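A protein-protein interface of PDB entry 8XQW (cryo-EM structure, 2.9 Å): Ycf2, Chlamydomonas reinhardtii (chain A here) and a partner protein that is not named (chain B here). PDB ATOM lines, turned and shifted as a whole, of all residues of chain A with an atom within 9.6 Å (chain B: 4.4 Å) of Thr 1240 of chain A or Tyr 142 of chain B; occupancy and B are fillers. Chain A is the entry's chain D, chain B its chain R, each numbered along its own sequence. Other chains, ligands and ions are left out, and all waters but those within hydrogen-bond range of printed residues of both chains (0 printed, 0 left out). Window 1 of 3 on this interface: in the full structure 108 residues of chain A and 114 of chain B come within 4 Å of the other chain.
Among the printed residues, merely in contact across the chains: Arg 988 of chain A with Tyr 141 of chain B (3.2 Å), Lys 1131 of chain A with Tyr 141 of chain B (3.7 Å), Trp 1235 of chain A with Tyr 142 of chain B (3.9 Å), Trp 1235 of chain A with Phe 270 of chain B (3.4 Å), Ala 1236 of chain A with Tyr 142 of chain B (3.5 Å), Ala 1236 of chain A with Ser 238 of chain B (3.9 Å), Lys 1239 of chain A with Leu 139 of chain B (3.6 Å), Lys 1239 of chain A with Tyr 142 of chain B (3.998 Å) and Thr 1240 of chain A with Tyr 142 of chain B (3.8 Å).
Thr 1240 of chain A touches just these residues of chain B: Tyr 142 (3.8 Å) and Lys 144 (3.4 Å). Of the printed residues of chain A, Tyr 142 of chain B touches Trp 1235, Ala 1236, Lys 1239 and Thr 1240. Of the printed residues of chain A, Phe 270 of chain B touches Trp 1235. Of the printed residues of chain B, Lys 1131 of chain A touches Tyr 141 (3.7 Å). Printed residues of chain A within 4 Å of Leu 139 of chain B: Lys 1239 (3.6 Å). Phe 1325 of chain A touches none of the printed residues of chain B. The nearest printed residue of chain B that does not touch Thr 1240 of chain A is Ala 145 of chain B (4.4 Å). The nearest printed residue of chain A that does not touch Tyr 142 of chain B is Arg 1232 of chain A (5.6 Å). The nearest printed residue of chain B that does not touch Lys 1131 of chain A is Leu 239 of chain B (5.5 Å).
The side-chain amide nitrogen of Asn 1241 of chain A sits close to the side-chain carboxylate of Asp 143 of chain B (2.4 Å). N of Lys 144 of chain B lies close to O of Thr 1240 of chain A (3.4 Å). The side-chain hydroxyl (OG) of Ser 238 of chain B is in hydrogen-bond range of the guanidinium group (NE) of Arg 1232 of chain A (3.3 Å).
The backbone carbonyl oxygen (O) of Ser 238 of chain B is in hydrogen-bond range of the side-chain hydroxyl (OH) of Tyr 142 of chain B, at 2.5 Å. The side-chain hydroxyl of Tyr 141 of chain B lies within hydrogen-bond range of the backbone carbonyl oxygen of Leu 239 of chain B (3.2 Å).
Hydrophobic or aromatic side chains of chain B within 4 Å of the printed part of chain A: Leu 139, Tyr 141, Tyr 142 and Phe 270. Of the 21 printed residues of chain A, 8 touch a printed residue of chain B. Hydrophobic or aromatic side chains of chain A that line the printed part of chain B: Trp 1235 and Ala 1236. Among the printed residues, 12 pairs touch across the chains. Among the printed residues, no Asp or Glu carboxylate lies within 4 Å of a Lys or Arg side-chain nitrogen of the other chain.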
ATOM      1  N   PHE A 984     -36.517 -24.577  27.621  1.00  0.00           N
ATOM      2  CA  PHE A 984     -35.306 -23.951  27.101  1.00  0.00           C
ATOM      3  C   PHE A 984     -35.319 -22.448  27.354  1.00  0.00           C
ATOM      4  O   PHE A 984     -34.320 -21.870  27.802  1.00  0.00           O
ATOM      5  CB  PHE A 984     -35.156 -24.240  25.612  1.00  0.00           C
ATOM      6  CG  PHE A 984     -34.038 -23.490  24.966  1.00  0.00           C
ATOM      7  CD1 PHE A 984     -32.751 -23.979  25.003  1.00  0.00           C
ATOM      8  CD2 PHE A 984     -34.271 -22.291  24.325  1.00  0.00           C
ATOM      9  CE1 PHE A 984     -31.718 -23.287  24.413  1.00  0.00           C
ATOM     10  CE2 PHE A 984     -33.243 -21.598  23.737  1.00  0.00           C
ATOM     11  CZ  PHE A 984     -31.966 -22.096  23.782  1.00  0.00           C
ATOM     12  N   ARG A 988     -32.674 -20.321  29.713  1.00  0.00           N
ATOM     13  CA  ARG A 988     -31.804 -19.321  29.111  1.00  0.00           C
ATOM     14  C   ARG A 988     -32.094 -17.909  29.590  1.00  0.00           C
ATOM     15  O   ARG A 988     -31.175 -17.088  29.645  1.00  0.00           O
ATOM     16  CB  ARG A 988     -31.911 -19.366  27.591  1.00  0.00           C
ATOM     17  CG  ARG A 988     -30.921 -20.303  26.964  1.00  0.00           C
ATOM     18  CD  ARG A 988     -29.997 -19.562  26.045  1.00  0.00           C
ATOM     19  NE  ARG A 988     -29.394 -18.399  26.681  1.00  0.00           N
ATOM     20  CZ  ARG A 988     -28.087 -18.178  26.722  1.00  0.00           C
ATOM     21  NH1 ARG A 988     -27.258 -19.040  26.165  1.00  0.00           N
ATOM     22  NH2 ARG A 988     -27.603 -17.101  27.316  1.00  0.00           N
ATOM     23  N   LYS A1131     -22.109 -15.821  11.088  1.00  0.00           N
ATOM     24  CA  LYS A1131     -21.992 -17.250  11.339  1.00  0.00           C
ATOM     25  C   LYS A1131     -22.360 -18.100  10.132  1.00  0.00           C
ATOM     26  O   LYS A1131     -21.982 -19.274  10.085  1.00  0.00           O
ATOM     27  CB  LYS A1131     -22.863 -17.657  12.529  1.00  0.00           C
ATOM     28  CG  LYS A1131     -22.210 -17.400  13.874  1.00  0.00           C
ATOM     29  CD  LYS A1131     -22.823 -18.246  14.972  1.00  0.00           C
ATOM     30  CE  LYS A1131     -22.165 -17.941  16.307  1.00  0.00           C
ATOM     31  NZ  LYS A1131     -22.672 -18.816  17.393  1.00  0.00           N
ATOM     32  N   ILE A1231      -7.738 -23.828  26.202  1.00  0.00           N
ATOM     33  CA  ILE A1231      -8.391 -24.560  27.282  1.00  0.00           C
ATOM     34  C   ILE A1231      -9.894 -24.308  27.265  1.00  0.00           C
ATOM     35  O   ILE A1231     -10.693 -25.223  27.500  1.00  0.00           O
ATOM     36  CB  ILE A1231      -7.766 -24.194  28.639  1.00  0.00           C
ATOM     37  CG1 ILE A1231      -6.306 -24.620  28.671  1.00  0.00           C
ATOM     38  CG2 ILE A1231      -8.503 -24.872  29.759  1.00  0.00           C
ATOM     39  CD1 ILE A1231      -5.481 -23.817  29.610  1.00  0.00           C
ATOM     40  N   ARG A1232     -10.302 -23.066  26.991  1.00  0.00           N
ATOM     41  CA  ARG A1232     -11.726 -22.763  26.889  1.00  0.00           C
ATOM     42  C   ARG A1232     -12.362 -23.522  25.740  1.00  0.00           C
ATOM     43  O   ARG A1232     -13.509 -23.968  25.835  1.00  0.00           O
ATOM     44  CB  ARG A1232     -11.934 -21.265  26.710  1.00  0.00           C
ATOM     45  CG  ARG A1232     -13.375 -20.873  26.490  1.00  0.00           C
ATOM     46  CD  ARG A1232     -13.500 -19.407  26.113  1.00  0.00           C
ATOM     47  NE  ARG A1232     -12.894 -19.119  24.822  1.00  0.00           N
ATOM     48  CZ  ARG A1232     -12.197 -18.024  24.555  1.00  0.00           C
ATOM     49  NH1 ARG A1232     -12.016 -17.109  25.491  1.00  0.00           N
ATOM     50  NH2 ARG A1232     -11.680 -17.845  23.353  1.00  0.00           N
ATOM     51  N   LEU A1233     -11.623 -23.689  24.650  1.00  0.00           N
ATOM     52  CA  LEU A1233     -12.123 -24.479  23.535  1.00  0.00           C
ATOM     53  C   LEU A1233     -12.401 -25.905  23.962  1.00  0.00           C
ATOM     54  O   LEU A1233     -13.461 -26.463  23.650  1.00  0.00           O
ATOM     55  CB  LEU A1233     -11.116 -24.457  22.394  1.00  0.00           C
ATOM     56  CG  LEU A1233     -11.557 -25.207  21.151  1.00  0.00           C
ATOM     57  CD1 LEU A1233     -12.735 -24.495  20.556  1.00  0.00           C
ATOM     58  CD2 LEU A1233     -10.425 -25.296  20.163  1.00  0.00           C
ATOM     59  N   ASN A1234     -11.460 -26.513  24.684  1.00  0.00           N
ATOM     60  CA  ASN A1234     -11.656 -27.893  25.126  1.00  0.00           C
ATOM     61  C   ASN A1234     -12.825 -28.013  26.092  1.00  0.00           C
ATOM     62  O   ASN A1234     -13.658 -28.920  25.969  1.00  0.00           O
ATOM     63  CB  ASN A1234     -10.389 -28.420  25.773  1.00  0.00           C
ATOM     64  CG  ASN A1234      -9.483 -29.090  24.789  1.00  0.00           C
ATOM     65  OD1 ASN A1234      -9.926 -29.564  23.748  1.00  0.00           O
ATOM     66  ND2 ASN A1234      -8.200 -29.140  25.110  1.00  0.00           N
ATOM     67  N   TRP A1235     -12.887 -27.128  27.081  1.00  0.00           N
ATOM     68  CA  TRP A1235     -13.993 -27.162  28.027  1.00  0.00           C
ATOM     69  C   TRP A1235     -15.329 -27.047  27.317  1.00  0.00           C
ATOM     70  O   TRP A1235     -16.265 -27.800  27.610  1.00  0.00           O
ATOM     71  CB  TRP A1235     -13.823 -26.047  29.046  1.00  0.00           C
ATOM     72  CG  TRP A1235     -14.920 -25.946  30.016  1.00  0.00           C
ATOM     73  CD1 TRP A1235     -15.093 -26.701  31.122  1.00  0.00           C
ATOM     74  CD2 TRP A1235     -16.005 -25.021  29.988  1.00  0.00           C
ATOM     75  NE1 TRP A1235     -16.221 -26.316  31.791  1.00  0.00           N
ATOM     76  CE2 TRP A1235     -16.802 -25.281  31.110  1.00  0.00           C
ATOM     77  CE3 TRP A1235     -16.383 -24.001  29.119  1.00  0.00           C
ATOM     78  CZ2 TRP A1235     -17.952 -24.562  31.387  1.00  0.00           C
ATOM     79  CZ3 TRP A1235     -17.519 -23.289  29.396  1.00  0.00           C
ATOM     80  CH2 TRP A1235     -18.293 -23.571  30.519  1.00  0.00           C
ATOM     81  N   ALA A1236     -15.434 -26.113  26.368  1.00  0.00           N
ATOM     82  CA  ALA A1236     -16.675 -25.930  25.630  1.00  0.00           C
ATOM     83  C   ALA A1236     -17.037 -27.157  24.815  1.00  0.00           C
ATOM     84  O   ALA A1236     -18.200 -27.558  24.795  1.00  0.00           O
ATOM     85  CB  ALA A1236     -16.561 -24.718  24.717  1.00  0.00           C
ATOM     86  N   LEU A1237     -16.067 -27.763  24.133  1.00  0.00           N
ATOM     87  CA  LEU A1237     -16.380 -28.955  23.358  1.00  0.00           C
ATOM     88  C   LEU A1237     -16.805 -30.109  24.254  1.00  0.00           C
ATOM     89  O   LEU A1237     -17.578 -30.970  23.827  1.00  0.00           O
ATOM     90  CB  LEU A1237     -15.189 -29.343  22.489  1.00  0.00           C
ATOM     91  CG  LEU A1237     -15.223 -30.737  21.872  1.00  0.00           C
ATOM     92  CD1 LEU A1237     -16.381 -30.873  20.927  1.00  0.00           C
ATOM     93  CD2 LEU A1237     -13.934 -31.039  21.156  1.00  0.00           C
ATOM     94  N   ASN A1238     -16.331 -30.147  25.500  1.00  0.00           N
ATOM     95  CA  ASN A1238     -16.812 -31.187  26.408  1.00  0.00           C
ATOM     96  C   ASN A1238     -18.219 -30.890  26.901  1.00  0.00           C
ATOM     97  O   ASN A1238     -19.009 -31.811  27.120  1.00  0.00           O
ATOM     98  CB  ASN A1238     -15.880 -31.346  27.602  1.00  0.00           C
ATOM     99  CG  ASN A1238     -16.427 -32.312  28.635  1.00  0.00           C
ATOM    100  OD1 ASN A1238     -17.196 -31.935  29.513  1.00  0.00           O
ATOM    101  ND2 ASN A1238     -16.029 -33.569  28.533  1.00  0.00           N
ATOM    102  N   LYS A1239     -18.545 -29.617  27.096  1.00  0.00           N
ATOM    103  CA  LYS A1239     -19.814 -29.278  27.734  1.00  0.00           C
ATOM    104  C   LYS A1239     -21.031 -29.555  26.869  1.00  0.00           C
ATOM    105  O   LYS A1239     -22.141 -29.244  27.304  1.00  0.00           O
ATOM    106  CB  LYS A1239     -19.820 -27.810  28.143  1.00  0.00           C
ATOM    107  CG  LYS A1239     -20.012 -27.603  29.618  1.00  0.00           C
ATOM    108  CD  LYS A1239     -19.168 -28.587  30.399  1.00  0.00           C
ATOM    109  CE  LYS A1239     -19.325 -28.406  31.887  1.00  0.00           C
ATOM    110  NZ  LYS A1239     -18.393 -29.287  32.626  1.00  0.00           N
ATOM    111  N   THR A1240     -20.870 -30.124  25.676  1.00  0.00           N
ATOM    112  CA  THR A1240     -22.005 -30.319  24.784  1.00  0.00           C
ATOM    113  C   THR A1240     -22.648 -31.688  24.914  1.00  0.00           C
ATOM    114  O   THR A1240     -23.589 -31.979  24.176  1.00  0.00           O
ATOM    115  CB  THR A1240     -21.583 -30.124  23.337  1.00  0.00           C
ATOM    116  OG1 THR A1240     -21.134 -31.372  22.810  1.00  0.00           O
ATOM    117  CG2 THR A1240     -20.467 -29.131  23.250  1.00  0.00           C
ATOM    118  N   ASN A1241     -22.158 -32.540  25.810  1.00  0.00           N
ATOM    119  CA  ASN A1241     -22.794 -33.821  26.108  1.00  0.00           C
ATOM    120  C   ASN A1241     -22.910 -34.707  24.871  1.00  0.00           C
ATOM    121  O   ASN A1241     -23.963 -35.281  24.606  1.00  0.00           O
ATOM    122  CB  ASN A1241     -24.164 -33.616  26.744  1.00  0.00           C
ATOM    123  CG  ASN A1241     -24.126 -32.640  27.880  1.00  0.00           C
ATOM    124  OD1 ASN A1241     -23.117 -32.515  28.568  1.00  0.00           O
ATOM    125  ND2 ASN A1241     -25.223 -31.931  28.085  1.00  0.00           N
ATOM    126  N   ILE A1242     -21.832 -34.822  24.105  1.00  0.00           N
ATOM    127  CA  ILE A1242     -21.805 -35.714  22.955  1.00  0.00           C
ATOM    128  C   ILE A1242     -20.713 -36.758  23.057  1.00  0.00           C
ATOM    129  O   ILE A1242     -20.548 -37.553  22.123  1.00  0.00           O
ATOM    130  CB  ILE A1242     -21.665 -34.931  21.637  1.00  0.00           C
ATOM    131  CG1 ILE A1242     -20.297 -34.264  21.562  1.00  0.00           C
ATOM    132  CG2 ILE A1242     -22.768 -33.907  21.496  1.00  0.00           C
ATOM    133  CD1 ILE A1242     -20.126 -33.401  20.355  1.00  0.00           C
ATOM    134  N   ASN A1243     -19.967 -36.794  24.156  1.00  0.00           N
ATOM    135  CA  ASN A1243     -18.813 -37.678  24.250  1.00  0.00           C
ATOM    136  C   ASN A1243     -19.171 -39.098  24.655  1.00  0.00           C
ATOM    137  O   ASN A1243     -18.410 -40.019  24.349  1.00  0.00           O
ATOM    138  CB  ASN A1243     -17.794 -37.108  25.233  1.00  0.00           C
ATOM    139  CG  ASN A1243     -18.369 -36.901  26.613  1.00  0.00           C
ATOM    140  OD1 ASN A1243     -19.502 -37.288  26.895  1.00  0.00           O
ATOM    141  ND2 ASN A1243     -17.590 -36.280  27.485  1.00  0.00           N
ATOM    142  N   THR A1244     -20.295 -39.301  25.330  1.00  0.00           N
ATOM    143  CA  THR A1244     -20.685 -40.641  25.729  1.00  0.00           C
ATOM    144  C   THR A1244     -21.291 -41.455  24.600  1.00  0.00           C
ATOM    145  O   THR A1244     -21.478 -42.663  24.767  1.00  0.00           O
ATOM    146  CB  THR A1244     -21.699 -40.587  26.867  1.00  0.00           C
ATOM    147  OG1 THR A1244     -22.068 -41.921  27.227  1.00  0.00           O
ATOM    148  CG2 THR A1244     -22.925 -39.852  26.409  1.00  0.00           C
ATOM    149  N   PHE A1245     -21.615 -40.834  23.471  1.00  0.00           N
ATOM    150  CA  PHE A1245     -22.297 -41.563  22.414  1.00  0.00           C
ATOM    151  C   PHE A1245     -21.330 -42.482  21.683  1.00  0.00           C
ATOM    152  O   PHE A1245     -20.366 -42.026  21.060  1.00  0.00           O
ATOM    153  CB  PHE A1245     -22.954 -40.608  21.425  1.00  0.00           C
ATOM    154  CG  PHE A1245     -23.684 -41.311  20.321  1.00  0.00           C
ATOM    155  CD1 PHE A1245     -24.934 -41.851  20.542  1.00  0.00           C
ATOM    156  CD2 PHE A1245     -23.112 -41.456  19.074  1.00  0.00           C
ATOM    157  CE1 PHE A1245     -25.606 -42.511  19.537  1.00  0.00           C
ATOM    158  CE2 PHE A1245     -23.779 -42.117  18.067  1.00  0.00           C
ATOM    159  CZ  PHE A1245     -25.028 -42.645  18.300  1.00  0.00           C
ATOM    160  N   PHE A1325     -13.981 -40.845  22.916  1.00  0.00           N
ATOM    161  CA  PHE A1325     -14.167 -39.502  22.386  1.00  0.00           C
ATOM    162  C   PHE A1325     -13.284 -38.544  23.165  1.00  0.00           C
ATOM    163  O   PHE A1325     -12.219 -38.934  23.649  1.00  0.00           O
ATOM    164  CB  PHE A1325     -15.620 -39.043  22.407  1.00  0.00           C
ATOM    165  CG  PHE A1325     -15.896 -37.948  21.411  1.00  0.00           C
ATOM    166  CD1 PHE A1325     -15.257 -37.950  20.184  1.00  0.00           C
ATOM    167  CD2 PHE A1325     -16.743 -36.904  21.711  1.00  0.00           C
ATOM    168  CE1 PHE A1325     -15.478 -36.944  19.274  1.00  0.00           C
ATOM    169  CE2 PHE A1325     -16.969 -35.897  20.800  1.00  0.00           C
ATOM    170  CZ  PHE A1325     -16.335 -35.918  19.584  1.00  0.00           C
ATOM    171  N   HIS A1326     -13.699 -37.287  23.266  1.00  0.00           N
ATOM    172  CA  HIS A1326     -12.899 -36.278  23.940  1.00  0.00           C
ATOM    173  C   HIS A1326     -12.772 -36.683  25.396  1.00  0.00           C
ATOM    174  O   HIS A1326     -13.458 -36.147  26.270  1.00  0.00           O
ATOM    175  CB  HIS A1326     -13.571 -34.913  23.826  1.00  0.00           C
ATOM    176  CG  HIS A1326     -12.640 -33.761  23.981  1.00  0.00           C
ATOM    177  ND1 HIS A1326     -13.024 -32.573  24.558  1.00  0.00           N
ATOM    178  CD2 HIS A1326     -11.347 -33.606  23.616  1.00  0.00           C
ATOM    179  CE1 HIS A1326     -12.003 -31.738  24.556  1.00  0.00           C
ATOM    180  NE2 HIS A1326     -10.974 -32.338  23.985  1.00  0.00           N
ATOM    181  N   TRP A1329      -9.982 -34.589  28.559  1.00  0.00           N
ATOM    182  CA  TRP A1329     -10.121 -33.136  28.295  1.00  0.00           C
ATOM    183  C   TRP A1329      -9.186 -32.315  29.170  1.00  0.00           C
ATOM    184  O   TRP A1329      -8.698 -31.313  28.646  1.00  0.00           O
ATOM    185  CB  TRP A1329     -11.589 -32.665  28.360  1.00  0.00           C
ATOM    186  CG  TRP A1329     -12.106 -31.892  29.547  1.00  0.00           C
ATOM    187  CD1 TRP A1329     -13.096 -32.327  30.375  1.00  0.00           C
ATOM    188  CD2 TRP A1329     -11.768 -30.562  30.000  1.00  0.00           C
ATOM    189  NE1 TRP A1329     -13.367 -31.391  31.334  1.00  0.00           N
ATOM    190  CE2 TRP A1329     -12.575 -30.298  31.127  1.00  0.00           C
ATOM    191  CE3 TRP A1329     -10.862 -29.579  29.593  1.00  0.00           C
ATOM    192  CZ2 TRP A1329     -12.496 -29.105  31.835  1.00  0.00           C
ATOM    193  CZ3 TRP A1329     -10.785 -28.400  30.295  1.00  0.00           C
ATOM    194  CH2 TRP A1329     -11.596 -28.165  31.399  1.00  0.00           C
ATOM    195  N   ARG B 138     -25.557 -20.166  31.406  1.00  0.00           N
ATOM    196  CA  ARG B 138     -24.458 -20.300  30.454  1.00  0.00           C
ATOM    197  C   ARG B 138     -24.346 -21.722  29.927  1.00  0.00           C
ATOM    198  O   ARG B 138     -23.890 -21.938  28.803  1.00  0.00           O
ATOM    199  CB  ARG B 138     -23.141 -19.879  31.091  1.00  0.00           C
ATOM    200  CG  ARG B 138     -23.014 -18.404  31.287  1.00  0.00           C
ATOM    201  CD  ARG B 138     -21.689 -18.047  31.902  1.00  0.00           C
ATOM    202  NE  ARG B 138     -21.773 -16.779  32.615  1.00  0.00           N
ATOM    203  CZ  ARG B 138     -21.558 -15.596  32.053  1.00  0.00           C
ATOM    204  NH1 ARG B 138     -21.240 -15.519  30.771  1.00  0.00           N
ATOM    205  NH2 ARG B 138     -21.660 -14.489  32.771  1.00  0.00           N
ATOM    206  N   LEU B 139     -24.737 -22.709  30.728  1.00  0.00           N
ATOM    207  CA  LEU B 139     -24.617 -24.091  30.286  1.00  0.00           C
ATOM    208  C   LEU B 139     -25.712 -24.483  29.312  1.00  0.00           C
ATOM    209  O   LEU B 139     -25.485 -25.351  28.468  1.00  0.00           O
ATOM    210  CB  LEU B 139     -24.633 -25.037  31.486  1.00  0.00           C
ATOM    211  CG  LEU B 139     -23.399 -25.062  32.385  1.00  0.00           C
ATOM    212  CD1 LEU B 139     -23.599 -26.026  33.531  1.00  0.00           C
ATOM    213  CD2 LEU B 139     -22.165 -25.427  31.597  1.00  0.00           C
ATOM    214  N   ALA B 140     -26.894 -23.874  29.417  1.00  0.00           N
ATOM    215  CA  ALA B 140     -27.971 -24.203  28.491  1.00  0.00           C
ATOM    216  C   ALA B 140     -27.612 -23.852  27.054  1.00  0.00           C
ATOM    217  O   ALA B 140     -28.187 -24.412  26.115  1.00  0.00           O
ATOM    218  CB  ALA B 140     -29.253 -23.488  28.904  1.00  0.00           C
ATOM    219  N   TYR B 141     -26.673 -22.928  26.861  1.00  0.00           N
ATOM    220  CA  TYR B 141     -26.215 -22.591  25.520  1.00  0.00           C
ATOM    221  C   TYR B 141     -25.585 -23.796  24.837  1.00  0.00           C
ATOM    222  O   TYR B 141     -26.108 -24.301  23.843  1.00  0.00           O
ATOM    223  CB  TYR B 141     -25.223 -21.442  25.601  1.00  0.00           C
ATOM    224  CG  TYR B 141     -24.501 -21.142  24.323  1.00  0.00           C
ATOM    225  CD1 TYR B 141     -25.120 -20.456  23.300  1.00  0.00           C
ATOM    226  CD2 TYR B 141     -23.190 -21.517  24.148  1.00  0.00           C
ATOM    227  CE1 TYR B 141     -24.456 -20.171  22.134  1.00  0.00           C
ATOM    228  CE2 TYR B 141     -22.520 -21.233  22.987  1.00  0.00           C
ATOM    229  CZ  TYR B 141     -23.155 -20.562  21.986  1.00  0.00           C
ATOM    230  OH  TYR B 141     -22.477 -20.284  20.830  1.00  0.00           O
ATOM    231  N   TYR B 142     -24.467 -24.284  25.375  1.00  0.00           N
ATOM    232  CA  TYR B 142     -23.743 -25.387  24.757  1.00  0.00           C
ATOM    233  C   TYR B 142     -24.547 -26.671  24.696  1.00  0.00           C
ATOM    234  O   TYR B 142     -24.316 -27.477  23.794  1.00  0.00           O
ATOM    235  CB  TYR B 142     -22.456 -25.681  25.518  1.00  0.00           C
ATOM    236  CG  TYR B 142     -21.536 -24.513  25.719  1.00  0.00           C
ATOM    237  CD1 TYR B 142     -20.558 -24.216  24.796  1.00  0.00           C
ATOM    238  CD2 TYR B 142     -21.623 -23.728  26.851  1.00  0.00           C
ATOM    239  CE1 TYR B 142     -19.710 -23.168  24.984  1.00  0.00           C
ATOM    240  CE2 TYR B 142     -20.781 -22.674  27.044  1.00  0.00           C
ATOM    241  CZ  TYR B 142     -19.825 -22.400  26.110  1.00  0.00           C
ATOM    242  OH  TYR B 142     -18.978 -21.343  26.298  1.00  0.00           O
ATOM    243  N   ASP B 143     -25.469 -26.873  25.631  1.00  0.00           N
ATOM    244  CA  ASP B 143     -26.137 -28.157  25.801  1.00  0.00           C
ATOM    245  C   ASP B 143     -26.729 -28.651  24.491  1.00  0.00           C
ATOM    246  O   ASP B 143     -27.650 -28.043  23.943  1.00  0.00           O
ATOM    247  CB  ASP B 143     -27.236 -28.029  26.848  1.00  0.00           C
ATOM    248  CG  ASP B 143     -27.519 -29.327  27.553  1.00  0.00           C
ATOM    249  OD1 ASP B 143     -26.761 -30.289  27.340  1.00  0.00           O
ATOM    250  OD2 ASP B 143     -28.497 -29.386  28.325  1.00  0.00           O
ATOM    251  N   LYS B 144     -26.205 -29.765  23.993  1.00  0.00           N
ATOM    252  CA  LYS B 144     -26.658 -30.338  22.734  1.00  0.00           C
ATOM    253  C   LYS B 144     -27.352 -31.672  22.940  1.00  0.00           C
ATOM    254  O   LYS B 144     -27.321 -32.520  22.046  1.00  0.00           O
ATOM    255  CB  LYS B 144     -25.490 -30.508  21.765  1.00  0.00           C
ATOM    256  CG  LYS B 144     -25.766 -30.009  20.373  1.00  0.00           C
ATOM    257  CD  LYS B 144     -25.844 -28.495  20.337  1.00  0.00           C
ATOM    258  CE  LYS B 144     -26.479 -28.007  19.044  1.00  0.00           C
ATOM    259  NZ  LYS B 144     -27.925 -28.352  18.996  1.00  0.00           N
ATOM    260  N   ALA B 145     -27.962 -31.886  24.106  1.00  0.00           N
ATOM    261  CA  ALA B 145     -28.645 -33.150  24.352  1.00  0.00           C
ATOM    262  C   ALA B 145     -29.915 -33.256  23.527  1.00  0.00           C
ATOM    263  O   ALA B 145     -30.162 -34.284  22.889  1.00  0.00           O
ATOM    264  CB  ALA B 145     -28.965 -33.298  25.836  1.00  0.00           C
ATOM    265  N   SER B 238     -17.235 -21.038  20.795  1.00  0.00           N
ATOM    266  CA  SER B 238     -17.007 -21.492  22.154  1.00  0.00           C
ATOM    267  C   SER B 238     -17.527 -20.518  23.185  1.00  0.00           C
ATOM    268  O   SER B 238     -17.546 -20.850  24.372  1.00  0.00           O
ATOM    269  CB  SER B 238     -15.516 -21.749  22.377  1.00  0.00           C
ATOM    270  OG  SER B 238     -14.815 -20.544  22.599  1.00  0.00           O
ATOM    271  N   LEU B 239     -17.967 -19.337  22.761  1.00  0.00           N
ATOM    272  CA  LEU B 239     -18.466 -18.323  23.666  1.00  0.00           C
ATOM    273  C   LEU B 239     -19.973 -18.186  23.513  1.00  0.00           C
ATOM    274  O   LEU B 239     -20.498 -18.311  22.404  1.00  0.00           O
ATOM    275  CB  LEU B 239     -17.800 -16.976  23.393  1.00  0.00           C
ATOM    276  CG  LEU B 239     -16.422 -16.788  24.008  1.00  0.00           C
ATOM    277  CD1 LEU B 239     -15.682 -15.673  23.312  1.00  0.00           C
ATOM    278  CD2 LEU B 239     -16.552 -16.502  25.487  1.00  0.00           C
ATOM    279  N   PRO B 240     -20.696 -17.946  24.600  1.00  0.00           N
ATOM    280  CA  PRO B 240     -22.131 -17.717  24.501  1.00  0.00           C
ATOM    281  C   PRO B 240     -22.414 -16.365  23.872  1.00  0.00           C
ATOM    282  O   PRO B 240     -21.492 -15.560  23.680  1.00  0.00           O
ATOM    283  CB  PRO B 240     -22.594 -17.765  25.965  1.00  0.00           C
ATOM    284  CG  PRO B 240     -21.491 -18.395  26.704  1.00  0.00           C
ATOM    285  CD  PRO B 240     -20.252 -17.995  25.996  1.00  0.00           C
ATOM    286  N   PHE B 270     -14.780 -15.347  33.167  1.00  0.00           N
ATOM    287  CA  PHE B 270     -15.271 -16.633  32.689  1.00  0.00           C
ATOM    288  C   PHE B 270     -14.122 -17.592  32.398  1.00  0.00           C
ATOM    289  O   PHE B 270     -14.112 -18.746  32.856  1.00  0.00           O
ATOM    290  CB  PHE B 270     -16.121 -16.405  31.447  1.00  0.00           C
ATOM    291  CG  PHE B 270     -16.654 -17.649  30.842  1.00  0.00           C
ATOM    292  CD1 PHE B 270     -17.740 -18.279  31.394  1.00  0.00           C
ATOM    293  CD2 PHE B 270     -16.085 -18.172  29.708  1.00  0.00           C
ATOM    294  CE1 PHE B 270     -18.240 -19.411  30.832  1.00  0.00           C
ATOM    295  CE2 PHE B 270     -16.580 -19.308  29.146  1.00  0.00           C
ATOM    296  CZ  PHE B 270     -17.661 -19.927  29.709  1.00  0.00           C
